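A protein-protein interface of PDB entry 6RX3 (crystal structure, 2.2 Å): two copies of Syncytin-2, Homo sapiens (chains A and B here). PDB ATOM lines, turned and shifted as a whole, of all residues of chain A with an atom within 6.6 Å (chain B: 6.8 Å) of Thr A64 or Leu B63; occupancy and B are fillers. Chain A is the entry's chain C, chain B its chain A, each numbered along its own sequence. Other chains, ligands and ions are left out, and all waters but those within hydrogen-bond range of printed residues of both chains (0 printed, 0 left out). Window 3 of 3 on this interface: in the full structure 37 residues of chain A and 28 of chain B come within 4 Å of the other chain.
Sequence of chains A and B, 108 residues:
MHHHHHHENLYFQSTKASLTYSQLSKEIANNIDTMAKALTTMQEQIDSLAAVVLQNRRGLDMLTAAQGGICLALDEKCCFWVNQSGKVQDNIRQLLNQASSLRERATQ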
ATOM      1  N   GLY A  59       5.702  -0.074  28.914  1.00  0.00           N
ATOM      2  CA  GLY A  59       4.646  -0.192  29.907  1.00  0.00           C
ATOM      3  C   GLY A  59       3.786  -1.430  29.702  1.00  0.00           C
ATOM      4  O   GLY A  59       3.539  -2.170  30.661  1.00  0.00           O
ATOM      5  N   LEU A  60       3.369  -1.692  28.436  1.00  0.00           N
ATOM      6  CA  LEU A  60       2.573  -2.866  28.052  1.00  0.00           C
ATOM      7  C   LEU A  60       3.388  -4.162  28.142  1.00  0.00           C
ATOM      8  O   LEU A  60       2.853  -5.197  28.553  1.00  0.00           O
ATOM      9  CB  LEU A  60       1.958  -2.709  26.649  1.00  0.00           C
ATOM     10  CG  LEU A  60       0.733  -1.803  26.554  1.00  0.00           C
ATOM     11  CD1 LEU A  60       0.558  -1.298  25.156  1.00  0.00           C
ATOM     12  CD2 LEU A  60      -0.558  -2.525  27.022  1.00  0.00           C
ATOM     13  N   ASP A  61       4.676  -4.105  27.765  1.00  0.00           N
ATOM     14  CA  ASP A  61       5.597  -5.242  27.869  1.00  0.00           C
ATOM     15  C   ASP A  61       5.803  -5.661  29.346  1.00  0.00           C
ATOM     16  O   ASP A  61       5.855  -6.856  29.637  1.00  0.00           O
ATOM     17  CB  ASP A  61       6.940  -4.950  27.166  1.00  0.00           C
ATOM     18  CG  ASP A  61       6.871  -5.048  25.647  1.00  0.00           C
ATOM     19  OD1 ASP A  61       5.961  -5.745  25.131  1.00  0.00           O
ATOM     20  OD2 ASP A  61       7.739  -4.460  24.977  1.00  0.00           O
ATOM     21  N   MET A  62       5.877  -4.678  30.256  1.00  0.00           N
ATOM     22  CA  MET A  62       6.029  -4.882  31.698  1.00  0.00           C
ATOM     23  C   MET A  62       4.768  -5.543  32.286  1.00  0.00           C
ATOM     24  O   MET A  62       4.885  -6.498  33.049  1.00  0.00           O
ATOM     25  CB  MET A  62       6.344  -3.553  32.408  1.00  0.00           C
ATOM     26  CG  MET A  62       6.483  -3.691  33.918  1.00  0.00           C
ATOM     27  SD  MET A  62       6.299  -2.139  34.832  1.00  0.00           S
ATOM     28  CE  MET A  62       4.476  -1.964  34.813  1.00  0.00           C
ATOM     29  N   LEU A  63       3.573  -5.052  31.904  1.00  0.00           N
ATOM     30  CA  LEU A  63       2.299  -5.604  32.356  1.00  0.00           C
ATOM     31  C   LEU A  63       2.053  -7.042  31.865  1.00  0.00           C
ATOM     32  O   LEU A  63       1.283  -7.762  32.492  1.00  0.00           O
ATOM     33  CB  LEU A  63       1.138  -4.692  31.936  1.00  0.00           C
ATOM     34  CG  LEU A  63       1.103  -3.284  32.543  1.00  0.00           C
ATOM     35  CD1 LEU A  63       0.047  -2.454  31.880  1.00  0.00           C
ATOM     36  CD2 LEU A  63       0.898  -3.319  34.062  1.00  0.00           C
ATOM     37  N   THR A  64       2.689  -7.450  30.746  1.00  0.00           N
ATOM     38  CA  THR A  64       2.551  -8.787  30.167  1.00  0.00           C
ATOM     39  C   THR A  64       3.882  -9.548  30.159  1.00  0.00           C
ATOM     40  O   THR A  64       4.022 -10.486  29.378  1.00  0.00           O
ATOM     41  CB  THR A  64       1.925  -8.727  28.754  1.00  0.00           C
ATOM     42  OG1 THR A  64       2.705  -7.863  27.938  1.00  0.00           O
ATOM     43  CG2 THR A  64       0.472  -8.293  28.760  1.00  0.00           C
ATOM     44  N   ALA A  65       4.838  -9.164  31.036  1.00  0.00           N
ATOM     45  CA  ALA A  65       6.177  -9.767  31.168  1.00  0.00           C
ATOM     46  C   ALA A  65       6.196 -11.302  31.233  1.00  0.00           C
ATOM     47  O   ALA A  65       7.023 -11.907  30.543  1.00  0.00           O
ATOM     48  CB  ALA A  65       6.913  -9.180  32.362  1.00  0.00           C
ATOM     49  N   ALA A  66       5.255 -11.925  31.993  1.00  0.00           N
ATOM     50  CA  ALA A  66       5.125 -13.398  32.131  1.00  0.00           C
ATOM     51  C   ALA A  66       4.721 -14.104  30.822  1.00  0.00           C
ATOM     52  O   ALA A  66       4.961 -15.305  30.664  1.00  0.00           O
ATOM     53  CB  ALA A  66       4.135 -13.746  33.243  1.00  0.00           C
ATOM     54  N   GLN A  67       4.108 -13.359  29.888  1.00  0.00           N
ATOM     55  CA  GLN A  67       3.700 -13.880  28.576  1.00  0.00           C
ATOM     56  C   GLN A  67       4.781 -13.577  27.529  1.00  0.00           C
ATOM     57  O   GLN A  67       4.670 -13.999  26.387  1.00  0.00           O
ATOM     58  CB  GLN A  67       2.349 -13.274  28.152  1.00  0.00           C
ATOM     59  CG  GLN A  67       1.176 -13.698  29.039  1.00  0.00           C
ATOM     60  CD  GLN A  67      -0.096 -13.019  28.616  1.00  0.00           C
ATOM     61  OE1 GLN A  67      -0.745 -13.423  27.645  1.00  0.00           O
ATOM     62  NE2 GLN A  67      -0.485 -11.972  29.332  1.00  0.00           N
ATOM     63  N   GLY A  68       5.811 -12.846  27.944  1.00  0.00           N
ATOM     64  CA  GLY A  68       6.925 -12.435  27.095  1.00  0.00           C
ATOM     65  C   GLY A  68       6.715 -11.110  26.373  1.00  0.00           C
ATOM     66  O   GLY A  68       7.328 -10.868  25.328  1.00  0.00           O
ATOM     67  N   GLY A  69       5.857 -10.256  26.917  1.00  0.00           N
ATOM     68  CA  GLY A  69       5.563  -8.973  26.293  1.00  0.00           C
ATOM     69  C   GLY A  69       4.228  -8.957  25.578  1.00  0.00           C
ATOM     70  O   GLY A  69       3.569  -9.995  25.436  1.00  0.00           O
ATOM     71  N   ILE A  70       3.824  -7.760  25.121  1.00  0.00           N
ATOM     72  CA  ILE A  70       2.514  -7.511  24.542  1.00  0.00           C
ATOM     73  C   ILE A  70       2.293  -8.226  23.207  1.00  0.00           C
ATOM     74  O   ILE A  70       1.193  -8.718  23.003  1.00  0.00           O
ATOM     75  CB  ILE A  70       2.165  -5.985  24.479  1.00  0.00           C
ATOM     76  CG1 ILE A  70       0.621  -5.743  24.458  1.00  0.00           C
ATOM     77  CG2 ILE A  70       2.879  -5.237  23.341  1.00  0.00           C
ATOM     78  CD1 ILE A  70      -0.179  -6.208  25.714  1.00  0.00           C
ATOM     79  N   CYS A  71       3.295  -8.294  22.324  1.00  0.00           N
ATOM     80  CA  CYS A  71       3.161  -8.936  21.010  1.00  0.00           C
ATOM     81  C   CYS A  71       2.891 -10.439  21.142  1.00  0.00           C
ATOM     82  O   CYS A  71       1.927 -10.924  20.548  1.00  0.00           O
ATOM     83  CB  CYS A  71       4.352  -8.613  20.110  1.00  0.00           C
ATOM     84  SG  CYS A  71       4.563  -6.835  19.780  1.00  0.00           S
ATOM     85  N   ALA A  73       1.640 -11.803  23.943  1.00  0.00           N
ATOM     86  CA  ALA A  73       0.352 -11.872  24.636  1.00  0.00           C
ATOM     87  C   ALA A  73      -0.793 -11.730  23.611  1.00  0.00           C
ATOM     88  O   ALA A  73      -1.782 -12.460  23.700  1.00  0.00           O
ATOM     89  CB  ALA A  73       0.258 -10.789  25.703  1.00  0.00           C
ATOM     90  N   ARG B  58      -4.664  -2.404  20.755  1.00  0.00           N
ATOM     91  CA  ARG B  58      -5.150  -3.796  20.762  1.00  0.00           C
ATOM     92  C   ARG B  58      -4.676  -4.513  22.033  1.00  0.00           C
ATOM     93  O   ARG B  58      -5.406  -5.337  22.572  1.00  0.00           O
ATOM     94  CB  ARG B  58      -4.689  -4.560  19.512  1.00  0.00           C
ATOM     95  CG  ARG B  58      -5.397  -4.134  18.227  1.00  0.00           C
ATOM     96  CD  ARG B  58      -5.203  -5.146  17.099  1.00  0.00           C
ATOM     97  NE  ARG B  58      -3.804  -5.329  16.696  1.00  0.00           N
ATOM     98  CZ  ARG B  58      -3.136  -4.520  15.878  1.00  0.00           C
ATOM     99  NH1 ARG B  58      -1.885  -4.798  15.535  1.00  0.00           N
ATOM    100  NH2 ARG B  58      -3.712  -3.429  15.396  1.00  0.00           N
ATOM    101  N   GLY B  59      -3.479  -4.152  22.500  1.00  0.00           N
ATOM    102  CA  GLY B  59      -2.883  -4.643  23.733  1.00  0.00           C
ATOM    103  C   GLY B  59      -3.708  -4.253  24.939  1.00  0.00           C
ATOM    104  O   GLY B  59      -4.016  -5.101  25.773  1.00  0.00           O
ATOM    105  N   LEU B  60      -4.122  -2.979  25.004  1.00  0.00           N
ATOM    106  CA  LEU B  60      -4.948  -2.416  26.081  1.00  0.00           C
ATOM    107  C   LEU B  60      -6.378  -2.949  26.041  1.00  0.00           C
ATOM    108  O   LEU B  60      -6.938  -3.215  27.100  1.00  0.00           O
ATOM    109  CB  LEU B  60      -4.937  -0.882  26.066  1.00  0.00           C
ATOM    110  CG  LEU B  60      -3.635  -0.203  26.489  1.00  0.00           C
ATOM    111  CD1 LEU B  60      -3.588   1.224  25.985  1.00  0.00           C
ATOM    112  CD2 LEU B  60      -3.464  -0.208  28.011  1.00  0.00           C
ATOM    113  N   ASP B  61      -6.961  -3.123  24.835  1.00  0.00           N
ATOM    114  CA  ASP B  61      -8.297  -3.702  24.677  1.00  0.00           C
ATOM    115  C   ASP B  61      -8.325  -5.184  25.122  1.00  0.00           C
ATOM    116  O   ASP B  61      -9.356  -5.658  25.602  1.00  0.00           O
ATOM    117  CB  ASP B  61      -8.800  -3.572  23.231  1.00  0.00           C
ATOM    118  CG  ASP B  61      -9.213  -2.169  22.834  1.00  0.00           C
ATOM    119  OD1 ASP B  61      -9.563  -1.365  23.741  1.00  0.00           O
ATOM    120  OD2 ASP B  61      -9.208  -1.873  21.616  1.00  0.00           O
ATOM    121  N   MET B  62      -7.199  -5.898  24.944  1.00  0.00           N
ATOM    122  CA  MET B  62      -7.041  -7.291  25.351  1.00  0.00           C
ATOM    123  C   MET B  62      -6.969  -7.364  26.896  1.00  0.00           C
ATOM    124  O   MET B  62      -7.602  -8.242  27.496  1.00  0.00           O
ATOM    125  CB  MET B  62      -5.799  -7.900  24.658  1.00  0.00           C
ATOM    126  CG  MET B  62      -5.490  -9.342  25.023  1.00  0.00           C
ATOM    127  SD  MET B  62      -4.395  -9.488  26.469  1.00  0.00           S
ATOM    128  CE  MET B  62      -2.862  -8.813  25.802  1.00  0.00           C
ATOM    129  N   LEU B  63      -6.204  -6.436  27.526  1.00  0.00           N
ATOM    130  CA  LEU B  63      -6.026  -6.373  28.983  1.00  0.00           C
ATOM    131  C   LEU B  63      -7.327  -6.000  29.721  1.00  0.00           C
ATOM    132  O   LEU B  63      -7.535  -6.452  30.850  1.00  0.00           O
ATOM    133  CB  LEU B  63      -4.888  -5.408  29.371  1.00  0.00           C
ATOM    134  CG  LEU B  63      -3.434  -5.816  29.032  1.00  0.00           C
ATOM    135  CD1 LEU B  63      -2.477  -4.703  29.391  1.00  0.00           C
ATOM    136  CD2 LEU B  63      -3.002  -7.079  29.782  1.00  0.00           C
ATOM    137  N   THR B  64      -8.197  -5.191  29.078  1.00  0.00           N
ATOM    138  CA  THR B  64      -9.505  -4.766  29.604  1.00  0.00           C
ATOM    139  C   THR B  64     -10.674  -5.433  28.818  1.00  0.00           C
ATOM    140  O   THR B  64     -11.747  -4.840  28.692  1.00  0.00           O
ATOM    141  CB  THR B  64      -9.607  -3.233  29.583  1.00  0.00           C
ATOM    142  OG1 THR B  64      -9.384  -2.792  28.249  1.00  0.00           O
ATOM    143  CG2 THR B  64      -8.629  -2.553  30.541  1.00  0.00           C
ATOM    144  N   ALA B  65     -10.463  -6.657  28.290  1.00  0.00           N
ATOM    145  CA  ALA B  65     -11.469  -7.397  27.513  1.00  0.00           C
ATOM    146  C   ALA B  65     -12.784  -7.633  28.285  1.00  0.00           C
ATOM    147  O   ALA B  65     -13.858  -7.523  27.685  1.00  0.00           O
ATOM    148  CB  ALA B  65     -10.902  -8.715  27.002  1.00  0.00           C
ATOM    149  N   ALA B  66     -12.695  -7.886  29.615  1.00  0.00           N
ATOM    150  CA  ALA B  66     -13.864  -8.085  30.486  1.00  0.00           C
ATOM    151  C   ALA B  66     -14.715  -6.817  30.578  1.00  0.00           C
ATOM    152  O   ALA B  66     -15.942  -6.924  30.663  1.00  0.00           O
ATOM    153  CB  ALA B  66     -13.435  -8.544  31.877  1.00  0.00           C
ATOM    154  N   GLN B  67     -14.070  -5.622  30.495  1.00  0.00           N
ATOM    155  CA  GLN B  67     -14.751  -4.319  30.517  1.00  0.00           C
ATOM    156  C   GLN B  67     -15.194  -3.835  29.128  1.00  0.00           C
ATOM    157  O   GLN B  67     -15.804  -2.772  29.017  1.00  0.00           O
ATOM    158  CB  GLN B  67     -13.903  -3.250  31.222  1.00  0.00           C
ATOM    159  CG  GLN B  67     -13.794  -3.446  32.725  1.00  0.00           C
ATOM    160  CD  GLN B  67     -12.672  -2.629  33.299  1.00  0.00           C
ATOM    161  OE1 GLN B  67     -11.494  -3.003  33.218  1.00  0.00           O
ATOM    162  NE2 GLN B  67     -13.011  -1.486  33.882  1.00  0.00           N
ATOM    163  N   ILE B  70     -10.463  -0.746  26.381  1.00  0.00           N
ATOM    164  CA  ILE B  70      -9.868   0.349  27.141  1.00  0.00           C
ATOM    165  C   ILE B  70     -10.730   1.628  27.138  1.00  0.00           C
ATOM    166  O   ILE B  70     -10.708   2.335  28.129  1.00  0.00           O
ATOM    167  CB  ILE B  70      -8.387   0.604  26.718  1.00  0.00           C
ATOM    168  CG1 ILE B  70      -7.579   1.339  27.819  1.00  0.00           C
ATOM    169  CG2 ILE B  70      -8.259   1.304  25.356  1.00  0.00           C
ATOM    170  CD1 ILE B  70      -7.270   0.529  29.087  1.00  0.00           C
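Leu A60 touches its own counterpart, Leu B60.
Leu A60 touches Leu B63, but with the chains exchanged Leu A63 does not touch Leu B60 (5.7 Å).
Ile A70 touches Gly B59, but with the chains exchanged Gly A59 does not touch Ile B70 (11.2 Å).
Ile A70 touches Met B62, but with the chains exchanged Met A62 does not touch Ile B70 (13.3 Å).
10 positions are printed for both chains.
The side-chain hydroxyl (OG1) of Thr B64 sits at hydrogen-bond distance from the backbone carbonyl oxygen (O) of Leu B60 (2.7 Å).
The backbone carbonyl oxygen (O) of Thr A64 sits at hydrogen-bond distance from the backbone NH (N) of Gly A69 (3.1 Å).
The backbone carbonyl oxygen of Leu A60 lies within hydrogen-bond range of the side-chain hydroxyl of Thr A64 (2.7 Å).
The backbone NH (N) of Ile A70 lies within hydrogen-bond range of the side-chain carboxylate (OD1) of Asp A61 (2.9 Å).
N of Ile A70 sits at hydrogen-bond distance from OG1 of Thr A64.
Among the printed residues, merely in contact across the chains: Leu A60 with Leu B60 (3.8 Å), Leu A60 with Leu B63 (3.7 Å), Thr A64 with Leu B63 (3.8 Å), Ile A70 with Gly B59 (3.7 Å), Ile A70 with Met B62 (3.7 Å) and Ala A73 with Met B62 (3.7 Å).
Of the 14 printed residues of chain A, 4 touch a printed residue of chain B.
Hydrophobic or aromatic side chains of chain A that line the printed part of chain B: Leu A60, Ile A70 and Ala A73.
Of the printed residues of chain B, Leu A60 touches Leu B60 and Leu B63.
Cys A71 touches none of the printed residues of chain B.
Printed residues of chain A within 4 Å of Leu B60: Leu A60.
Printed residues of chain A within 4 Å of Met B62: Ile A70 (3.7 Å) and Ala A73 (3.7 Å).
Ala B66 touches none of the printed residues of chain A.
The nearest printed residue of chain A that does not touch Leu B60 is Ile A70 (5.1 Å).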
